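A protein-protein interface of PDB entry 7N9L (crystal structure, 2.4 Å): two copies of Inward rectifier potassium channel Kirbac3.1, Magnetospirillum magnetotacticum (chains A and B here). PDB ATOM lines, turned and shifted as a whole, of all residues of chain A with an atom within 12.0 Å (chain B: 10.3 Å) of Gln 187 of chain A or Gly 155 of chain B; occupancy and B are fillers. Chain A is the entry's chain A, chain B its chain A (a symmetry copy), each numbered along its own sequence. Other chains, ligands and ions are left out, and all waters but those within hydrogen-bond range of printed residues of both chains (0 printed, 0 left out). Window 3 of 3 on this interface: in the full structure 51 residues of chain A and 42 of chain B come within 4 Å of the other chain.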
ATOM      1  N   SER A 183      18.587 -40.890  -8.475  1.00  0.00           N
ATOM      2  CA  SER A 183      17.654 -40.827  -7.358  1.00  0.00           C
ATOM      3  C   SER A 183      18.430 -40.674  -6.057  1.00  0.00           C
ATOM      4  O   SER A 183      19.346 -41.452  -5.772  1.00  0.00           O
ATOM      5  CB  SER A 183      16.783 -42.079  -7.321  1.00  0.00           C
ATOM      6  OG  SER A 183      16.220 -42.327  -8.597  1.00  0.00           O
ATOM      7  N   GLU A 184      18.072 -39.661  -5.277  1.00  0.00           N
ATOM      8  CA  GLU A 184      18.749 -39.355  -4.028  1.00  0.00           C
ATOM      9  C   GLU A 184      17.727 -39.249  -2.908  1.00  0.00           C
ATOM     10  O   GLU A 184      16.526 -39.128  -3.148  1.00  0.00           O
ATOM     11  CB  GLU A 184      19.547 -38.052  -4.130  1.00  0.00           C
ATOM     12  CG  GLU A 184      20.788 -38.159  -4.987  1.00  0.00           C
ATOM     13  CD  GLU A 184      21.798 -37.075  -4.677  1.00  0.00           C
ATOM     14  OE1 GLU A 184      21.438 -36.110  -3.969  1.00  0.00           O
ATOM     15  OE2 GLU A 184      22.953 -37.193  -5.133  1.00  0.00           O
ATOM     16  N   ILE A 185      18.227 -39.288  -1.675  1.00  0.00           N
ATOM     17  CA  ILE A 185      17.404 -39.176  -0.476  1.00  0.00           C
ATOM     18  C   ILE A 185      17.917 -38.002   0.346  1.00  0.00           C
ATOM     19  O   ILE A 185      19.119 -37.909   0.619  1.00  0.00           O
ATOM     20  CB  ILE A 185      17.431 -40.468   0.362  1.00  0.00           C
ATOM     21  CG1 ILE A 185      17.210 -41.697  -0.519  1.00  0.00           C
ATOM     22  CG2 ILE A 185      16.368 -40.402   1.457  1.00  0.00           C
ATOM     23  CD1 ILE A 185      17.339 -43.014   0.226  1.00  0.00           C
ATOM     24  N   SER A 186      17.008 -37.116   0.743  1.00  0.00           N
ATOM     25  CA  SER A 186      17.367 -35.995   1.594  1.00  0.00           C
ATOM     26  C   SER A 186      17.444 -36.444   3.054  1.00  0.00           C
ATOM     27  O   SER A 186      16.990 -37.532   3.424  1.00  0.00           O
ATOM     28  CB  SER A 186      16.357 -34.859   1.441  1.00  0.00           C
ATOM     29  OG  SER A 186      15.102 -35.214   1.995  1.00  0.00           O
ATOM     30  N   GLN A 187      18.033 -35.588   3.894  1.00  0.00           N
ATOM     31  CA  GLN A 187      18.116 -35.906   5.316  1.00  0.00           C
ATOM     32  C   GLN A 187      16.775 -35.762   6.023  1.00  0.00           C
ATOM     33  O   GLN A 187      16.677 -36.113   7.203  1.00  0.00           O
ATOM     34  CB  GLN A 187      19.175 -35.038   6.007  1.00  0.00           C
ATOM     35  CG  GLN A 187      19.144 -33.560   5.673  1.00  0.00           C
ATOM     36  CD  GLN A 187      20.405 -32.842   6.127  1.00  0.00           C
ATOM     37  OE1 GLN A 187      20.543 -32.479   7.296  1.00  0.00           O
ATOM     38  NE2 GLN A 187      21.336 -32.641   5.201  1.00  0.00           N
ATOM     39  N   GLU A 188      15.751 -35.255   5.340  1.00  0.00           N
ATOM     40  CA  GLU A 188      14.375 -35.363   5.805  1.00  0.00           C
ATOM     41  C   GLU A 188      13.712 -36.652   5.334  1.00  0.00           C
ATOM     42  O   GLU A 188      12.530 -36.868   5.624  1.00  0.00           O
ATOM     43  CB  GLU A 188      13.549 -34.163   5.328  1.00  0.00           C
ATOM     44  CG  GLU A 188      13.997 -32.820   5.892  1.00  0.00           C
ATOM     45  CD  GLU A 188      15.182 -32.229   5.151  1.00  0.00           C
ATOM     46  OE1 GLU A 188      15.309 -32.467   3.930  1.00  0.00           O
ATOM     47  OE2 GLU A 188      15.988 -31.522   5.794  1.00  0.00           O
ATOM     48  N   GLY A 189      14.438 -37.502   4.613  1.00  0.00           N
ATOM     49  CA  GLY A 189      13.897 -38.743   4.109  1.00  0.00           C
ATOM     50  C   GLY A 189      13.203 -38.652   2.771  1.00  0.00           C
ATOM     51  O   GLY A 189      12.598 -39.640   2.340  1.00  0.00           O
ATOM     52  N   MET A 190      13.268 -37.505   2.099  1.00  0.00           N
ATOM     53  CA  MET A 190      12.599 -37.344   0.815  1.00  0.00           C
ATOM     54  C   MET A 190      13.467 -37.898  -0.308  1.00  0.00           C
ATOM     55  O   MET A 190      14.633 -37.520  -0.448  1.00  0.00           O
ATOM     56  CB  MET A 190      12.283 -35.872   0.555  1.00  0.00           C
ATOM     57  CG  MET A 190      11.923 -35.575  -0.893  1.00  0.00           C
ATOM     58  SD  MET A 190      10.685 -34.278  -1.074  1.00  0.00           S
ATOM     59  CE  MET A 190      10.276 -34.451  -2.811  1.00  0.00           C
ATOM     60  N   VAL A 191      12.893 -38.790  -1.112  1.00  0.00           N
ATOM     61  CA  VAL A 191      13.582 -39.388  -2.251  1.00  0.00           C
ATOM     62  C   VAL A 191      13.201 -38.608  -3.503  1.00  0.00           C
ATOM     63  O   VAL A 191      12.015 -38.363  -3.755  1.00  0.00           O
ATOM     64  CB  VAL A 191      13.228 -40.878  -2.399  1.00  0.00           C
ATOM     65  CG1 VAL A 191      14.096 -41.528  -3.468  1.00  0.00           C
ATOM     66  CG2 VAL A 191      13.391 -41.587  -1.069  1.00  0.00           C
ATOM     67  N   PHE A 192      14.202 -38.222  -4.290  1.00  0.00           N
ATOM     68  CA  PHE A 192      13.986 -37.350  -5.434  1.00  0.00           C
ATOM     69  C   PHE A 192      15.091 -37.571  -6.453  1.00  0.00           C
ATOM     70  O   PHE A 192      16.155 -38.109  -6.137  1.00  0.00           O
ATOM     71  CB  PHE A 192      13.943 -35.873  -5.006  1.00  0.00           C
ATOM     72  CG  PHE A 192      15.204 -35.400  -4.324  1.00  0.00           C
ATOM     73  CD1 PHE A 192      15.456 -35.716  -2.996  1.00  0.00           C
ATOM     74  CD2 PHE A 192      16.132 -34.631  -5.010  1.00  0.00           C
ATOM     75  CE1 PHE A 192      16.614 -35.279  -2.368  1.00  0.00           C
ATOM     76  CE2 PHE A 192      17.290 -34.192  -4.387  1.00  0.00           C
ATOM     77  CZ  PHE A 192      17.530 -34.517  -3.064  1.00  0.00           C
ATOM     78  N   ARG A 194      17.922 -35.932  -8.469  1.00  0.00           N
ATOM     79  CA  ARG A 194      18.764 -34.748  -8.422  1.00  0.00           C
ATOM     80  C   ARG A 194      19.637 -34.686  -9.670  1.00  0.00           C
ATOM     81  O   ARG A 194      20.016 -35.712 -10.240  1.00  0.00           O
ATOM     82  CB  ARG A 194      19.639 -34.735  -7.166  1.00  0.00           C
ATOM     83  CG  ARG A 194      20.223 -33.364  -6.853  1.00  0.00           C
ATOM     84  CD  ARG A 194      20.914 -33.353  -5.506  1.00  0.00           C
ATOM     85  NE  ARG A 194      20.535 -32.180  -4.730  1.00  0.00           N
ATOM     86  CZ  ARG A 194      20.444 -32.157  -3.409  1.00  0.00           C
ATOM     87  NH1 ARG A 194      20.695 -33.232  -2.679  1.00  0.00           N
ATOM     88  NH2 ARG A 194      20.081 -31.029  -2.803  1.00  0.00           N
ATOM     89  N   SER B 151      10.218 -24.302   3.739  1.00  0.00           N
ATOM     90  CA  SER B 151      10.224 -25.553   4.482  1.00  0.00           C
ATOM     91  C   SER B 151      11.646 -26.096   4.489  1.00  0.00           C
ATOM     92  O   SER B 151      12.507 -25.652   3.726  1.00  0.00           O
ATOM     93  CB  SER B 151       9.243 -26.563   3.880  1.00  0.00           C
ATOM     94  OG  SER B 151       9.528 -26.803   2.515  1.00  0.00           O
ATOM     95  N   ASP B 152      11.881 -27.063   5.371  1.00  0.00           N
ATOM     96  CA  ASP B 152      13.220 -27.610   5.538  1.00  0.00           C
ATOM     97  C   ASP B 152      13.577 -28.502   4.359  1.00  0.00           C
ATOM     98  O   ASP B 152      12.813 -29.396   3.987  1.00  0.00           O
ATOM     99  CB  ASP B 152      13.317 -28.405   6.840  1.00  0.00           C
ATOM    100  CG  ASP B 152      13.289 -27.522   8.072  1.00  0.00           C
ATOM    101  OD1 ASP B 152      13.612 -26.320   7.956  1.00  0.00           O
ATOM    102  OD2 ASP B 152      12.950 -28.031   9.161  1.00  0.00           O
ATOM    103  N   PHE B 153      14.744 -28.254   3.773  1.00  0.00           N
ATOM    104  CA  PHE B 153      15.298 -29.125   2.747  1.00  0.00           C
ATOM    105  C   PHE B 153      16.786 -29.272   3.019  1.00  0.00           C
ATOM    106  O   PHE B 153      17.498 -28.270   3.142  1.00  0.00           O
ATOM    107  CB  PHE B 153      15.056 -28.574   1.339  1.00  0.00           C
ATOM    108  CG  PHE B 153      15.548 -29.482   0.250  1.00  0.00           C
ATOM    109  CD1 PHE B 153      14.885 -30.663  -0.037  1.00  0.00           C
ATOM    110  CD2 PHE B 153      16.680 -29.162  -0.477  1.00  0.00           C
ATOM    111  CE1 PHE B 153      15.341 -31.505  -1.034  1.00  0.00           C
ATOM    112  CE2 PHE B 153      17.138 -29.999  -1.475  1.00  0.00           C
ATOM    113  CZ  PHE B 153      16.469 -31.171  -1.754  1.00  0.00           C
ATOM    114  N   GLU B 154      17.246 -30.516   3.130  1.00  0.00           N
ATOM    115  CA  GLU B 154      18.640 -30.813   3.455  1.00  0.00           C
ATOM    116  C   GLU B 154      19.065 -30.135   4.756  1.00  0.00           C
ATOM    117  O   GLU B 154      20.217 -29.722   4.908  1.00  0.00           O
ATOM    118  CB  GLU B 154      19.571 -30.400   2.312  1.00  0.00           C
ATOM    119  CG  GLU B 154      19.242 -31.042   0.974  1.00  0.00           C
ATOM    120  CD  GLU B 154      19.694 -32.487   0.883  1.00  0.00           C
ATOM    121  OE1 GLU B 154      19.631 -33.205   1.903  1.00  0.00           O
ATOM    122  OE2 GLU B 154      20.119 -32.902  -0.215  1.00  0.00           O
ATOM    123  N   GLY B 155      18.134 -30.007   5.701  1.00  0.00           N
ATOM    124  CA  GLY B 155      18.439 -29.444   6.999  1.00  0.00           C
ATOM    125  C   GLY B 155      18.447 -27.936   7.074  1.00  0.00           C
ATOM    126  O   GLY B 155      18.946 -27.386   8.062  1.00  0.00           O
ATOM    127  N   LYS B 156      17.913 -27.246   6.070  1.00  0.00           N
ATOM    128  CA  LYS B 156      17.871 -25.792   6.064  1.00  0.00           C
ATOM    129  C   LYS B 156      16.490 -25.319   5.639  1.00  0.00           C
ATOM    130  O   LYS B 156      15.905 -25.880   4.705  1.00  0.00           O
ATOM    131  CB  LYS B 156      18.927 -25.218   5.107  1.00  0.00           C
ATOM    132  CG  LYS B 156      20.258 -24.896   5.758  1.00  0.00           C
ATOM    133  CD  LYS B 156      21.409 -25.054   4.773  1.00  0.00           C
ATOM    134  CE  LYS B 156      22.720 -24.578   5.376  1.00  0.00           C
ATOM    135  NZ  LYS B 156      23.896 -25.270   4.776  1.00  0.00           N
ATOM    136  N   PRO B 157      15.931 -24.307   6.305  1.00  0.00           N
ATOM    137  CA  PRO B 157      14.708 -23.685   5.779  1.00  0.00           C
ATOM    138  C   PRO B 157      14.983 -23.096   4.404  1.00  0.00           C
ATOM    139  O   PRO B 157      15.943 -22.347   4.212  1.00  0.00           O
ATOM    140  CB  PRO B 157      14.372 -22.609   6.819  1.00  0.00           C
ATOM    141  CG  PRO B 157      15.632 -22.387   7.587  1.00  0.00           C
ATOM    142  CD  PRO B 157      16.356 -23.698   7.580  1.00  0.00           C
ATOM    143  N   THR B 158      14.139 -23.458   3.439  1.00  0.00           N
ATOM    144  CA  THR B 158      14.396 -23.185   2.030  1.00  0.00           C
ATOM    145  C   THR B 158      13.159 -22.577   1.387  1.00  0.00           C
ATOM    146  O   THR B 158      12.085 -23.186   1.401  1.00  0.00           O
ATOM    147  CB  THR B 158      14.799 -24.470   1.297  1.00  0.00           C
ATOM    148  OG1 THR B 158      15.960 -25.034   1.920  1.00  0.00           O
ATOM    149  CG2 THR B 158      15.094 -24.190  -0.168  1.00  0.00           C
ATOM    150  N   MET B 160      10.992 -21.821  -1.771  1.00  0.00           N
ATOM    151  CA  MET B 160      10.834 -22.550  -3.018  1.00  0.00           C
ATOM    152  C   MET B 160       9.645 -22.039  -3.814  1.00  0.00           C
ATOM    153  O   MET B 160       8.627 -21.634  -3.246  1.00  0.00           O
ATOM    154  CB  MET B 160      10.630 -24.053  -2.778  1.00  0.00           C
ATOM    155  CG  MET B 160      11.539 -24.673  -1.748  1.00  0.00           C
ATOM    156  SD  MET B 160      11.290 -26.461  -1.712  1.00  0.00           S
ATOM    157  CE  MET B 160      12.285 -26.902  -0.291  1.00  0.00           C
ATOM    158  N   MET B 215      14.999 -23.391  -5.690  1.00  0.00           N
ATOM    159  CA  MET B 215      15.244 -23.433  -4.252  1.00  0.00           C
ATOM    160  C   MET B 215      16.260 -22.390  -3.817  1.00  0.00           C
ATOM    161  O   MET B 215      17.328 -22.259  -4.427  1.00  0.00           O
ATOM    162  CB  MET B 215      15.738 -24.817  -3.821  1.00  0.00           C
ATOM    163  CG  MET B 215      14.685 -25.907  -3.882  1.00  0.00           C
ATOM    164  SD  MET B 215      15.334 -27.498  -3.331  1.00  0.00           S
ATOM    165  CE  MET B 215      13.897 -28.550  -3.491  1.00  0.00           C
ATOM    166  N   HIS B 216      15.935 -21.678  -2.744  1.00  0.00           N
ATOM    167  CA  HIS B 216      16.844 -20.720  -2.115  1.00  0.00           C
ATOM    168  C   HIS B 216      17.057 -21.127  -0.664  1.00  0.00           C
ATOM    169  O   HIS B 216      16.202 -20.845   0.196  1.00  0.00           O
ATOM    170  CB  HIS B 216      16.283 -19.301  -2.195  1.00  0.00           C
ATOM    171  CG  HIS B 216      16.914 -18.346  -1.229  1.00  0.00           C
ATOM    172  ND1 HIS B 216      18.198 -17.868  -1.384  1.00  0.00           N
ATOM    173  CD2 HIS B 216      16.437 -17.782  -0.094  1.00  0.00           C
ATOM    174  CE1 HIS B 216      18.484 -17.051  -0.386  1.00  0.00           C
ATOM    175  NE2 HIS B 216      17.432 -16.981   0.410  1.00  0.00           N
ATOM    176  N   PRO B 217      18.156 -21.806  -0.340  1.00  0.00           N
ATOM    177  CA  PRO B 217      18.429 -22.130   1.070  1.00  0.00           C
ATOM    178  C   PRO B 217      18.613 -20.857   1.881  1.00  0.00           C
ATOM    179  O   PRO B 217      19.448 -20.009   1.560  1.00  0.00           O
ATOM    180  CB  PRO B 217      19.719 -22.961   1.008  1.00  0.00           C
ATOM    181  CG  PRO B 217      19.788 -23.471  -0.400  1.00  0.00           C
ATOM    182  CD  PRO B 217      19.153 -22.401  -1.250  1.00  0.00           C
ATOM    183  N   ILE B 218      17.809 -20.718   2.930  1.00  0.00           N
ATOM    184  CA  ILE B 218      17.903 -19.557   3.806  1.00  0.00           C
ATOM    185  C   ILE B 218      18.992 -19.838   4.835  1.00  0.00           C
ATOM    186  O   ILE B 218      18.710 -20.260   5.961  1.00  0.00           O
ATOM    187  CB  ILE B 218      16.558 -19.238   4.475  1.00  0.00           C
ATOM    188  CG1 ILE B 218      15.489 -18.976   3.412  1.00  0.00           C
ATOM    189  CG2 ILE B 218      16.693 -18.015   5.371  1.00  0.00           C
ATOM    190  CD1 ILE B 218      14.086 -19.313   3.853  1.00  0.00           C
ATOM    191  N   ASP B 219      20.246 -19.630   4.436  1.00  0.00           N
ATOM    192  CA  ASP B 219      21.386 -19.762   5.323  1.00  0.00           C
ATOM    193  C   ASP B 219      21.733 -18.392   5.899  1.00  0.00           C
ATOM    194  O   ASP B 219      21.121 -17.374   5.562  1.00  0.00           O
ATOM    195  CB  ASP B 219      22.568 -20.383   4.581  1.00  0.00           C
ATOM    196  CG  ASP B 219      23.243 -19.416   3.628  1.00  0.00           C
ATOM    197  OD1 ASP B 219      22.628 -18.392   3.270  1.00  0.00           O
ATOM    198  OD2 ASP B 219      24.396 -19.683   3.233  1.00  0.00           O
ATOM    199  N   HIS B 220      22.748 -18.352   6.764  1.00  0.00           N
ATOM    200  CA  HIS B 220      23.059 -17.142   7.509  1.00  0.00           C
ATOM    201  C   HIS B 220      23.488 -15.997   6.600  1.00  0.00           C
ATOM    202  O   HIS B 220      23.688 -14.874   7.072  1.00  0.00           O
ATOM    203  CB  HIS B 220      24.140 -17.417   8.566  1.00  0.00           C
ATOM    204  CG  HIS B 220      25.357 -18.112   8.038  1.00  0.00           C
ATOM    205  ND1 HIS B 220      26.119 -18.962   8.811  1.00  0.00           N
ATOM    206  CD2 HIS B 220      25.948 -18.081   6.819  1.00  0.00           C
ATOM    207  CE1 HIS B 220      27.124 -19.428   8.090  1.00  0.00           C
ATOM    208  NE2 HIS B 220      27.044 -18.909   6.878  1.00  0.00           N
ATOM    209  N   TYR B 225      17.215 -14.355   6.079  1.00  0.00           N
ATOM    210  CA  TYR B 225      17.605 -15.136   7.246  1.00  0.00           C
ATOM    211  C   TYR B 225      17.107 -14.444   8.508  1.00  0.00           C
ATOM    212  O   TYR B 225      17.436 -13.280   8.756  1.00  0.00           O
ATOM    213  CB  TYR B 225      19.121 -15.299   7.275  1.00  0.00           C
ATOM    214  CG  TYR B 225      19.653 -16.062   8.465  1.00  0.00           C
ATOM    215  CD1 TYR B 225      19.527 -17.442   8.543  1.00  0.00           C
ATOM    216  CD2 TYR B 225      20.304 -15.404   9.500  1.00  0.00           C
ATOM    217  CE1 TYR B 225      20.022 -18.144   9.625  1.00  0.00           C
ATOM    218  CE2 TYR B 225      20.804 -16.096  10.582  1.00  0.00           C
ATOM    219  CZ  TYR B 225      20.661 -17.466  10.640  1.00  0.00           C
ATOM    220  OH  TYR B 225      21.154 -18.163  11.717  1.00  0.00           O
ATOM    221  N   HIS B 270       4.832 -27.771   1.541  1.00  0.00           N
ATOM    222  CA  HIS B 270       5.586 -28.709   0.719  1.00  0.00           C
ATOM    223  C   HIS B 270       4.824 -28.910  -0.582  1.00  0.00           C
ATOM    224  O   HIS B 270       3.637 -29.252  -0.557  1.00  0.00           O
ATOM    225  CB  HIS B 270       5.786 -30.058   1.422  1.00  0.00           C
ATOM    226  CG  HIS B 270       6.550 -29.972   2.707  1.00  0.00           C
ATOM    227  ND1 HIS B 270       5.955 -29.650   3.908  1.00  0.00           N
ATOM    228  CD2 HIS B 270       7.861 -30.178   2.982  1.00  0.00           C
ATOM    229  CE1 HIS B 270       6.865 -29.657   4.866  1.00  0.00           C
ATOM    230  NE2 HIS B 270       8.030 -29.974   4.330  1.00  0.00           N
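The backbone carbonyl oxygen of Glu 154 of chain B is in hydrogen-bond range of the side-chain amide nitrogen of Gln 187 of chain A, 3.1 Å away. OE1 of Glu 188 of chain A is in hydrogen-bond range of N of Glu 154 of chain B (2.9 Å). The side-chain carboxylate (OE2) of Glu 188 of chain A sits at hydrogen-bond distance from the backbone NH (N) of Gly 155 of chain B, at 2.6 Å. OE2 of Glu 154 of chain B lies within salt-bridge range of NH1 of Arg 194 of chain A, 2.6 Å away.
The backbone NH of Glu 184 of chain A sits at hydrogen-bond distance from the backbone carbonyl oxygen of Phe 192 of chain A (2.6 Å). NH1 of Arg 194 of chain A is in salt-bridge range of OE1 of Glu 184 of chain A, at 3.2 Å. OG of Ser 186 of chain A is in hydrogen-bond range of OE1 of Glu 188 of chain A (3.4 Å). The backbone NH (N) of Met 190 of chain A lies within hydrogen-bond range of the side-chain hydroxyl (OG) of Ser 186 of chain A, at 2.9 Å.
CA of Ser 186 of chain A touches OE1 of Glu 154 of chain B (3.6 Å). Gln 187 of chain A touches Gly 155 of chain B. CD of Glu 188 of chain A touches O of Asp 152 of chain B, at 3.9 Å. Phe 153 of chain B touches Glu 188 of chain A. CZ of Phe 153 of chain B touches CZ of Phe 192 of chain A, 3.7 Å away. NH2 of Arg 194 of chain A touches CE2 of Phe 153 of chain B, at 3.4 Å.
Of chain B, only Glu 154 (3.6 Å) comes within 4 Å of Ser 186 of chain A. Of the printed residues of chain B, Phe 192 of chain A touches Phe 153 (3.7 Å). Of the printed residues of chain B, Arg 194 of chain A touches Phe 153 (3.4 Å) and Glu 154 (2.6 Å). Asp 152 of chain B touches just one residue of chain A: Glu 188. Gly 155 of chain B touches just these residues of chain A: Gln 187 (3.7 Å) and Glu 188 (2.6 Å). No residue of chain A comes within 4 Å of Pro 157 of chain B. Asp 219 of chain B touches none of the printed residues of chain A. His 270 of chain B touches none of the printed residues of chain A. The nearest residue of chain A that does not touch Gly 155 of chain B is Ser 186 of chain A (6.7 Å).
Of the 17 printed residues of chain B, 4 touch a printed residue of chain A. Of the 11 printed residues of chain A, 5 touch a printed residue of chain B. Printed residues of chain A that touch a printed residue of chain B: Ser 186, Gln 187, Glu 188, Phe 192 and Arg 194. Along chain A the printed residues that touch a printed residue of chain B span positions 186 to 194. Among the printed residues, 10 pairs touch across the chains.
No position is printed for both chains. Of the 10 pairs that touch across the chains among the printed residues, none has its exchanged pair printed and touching as well.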
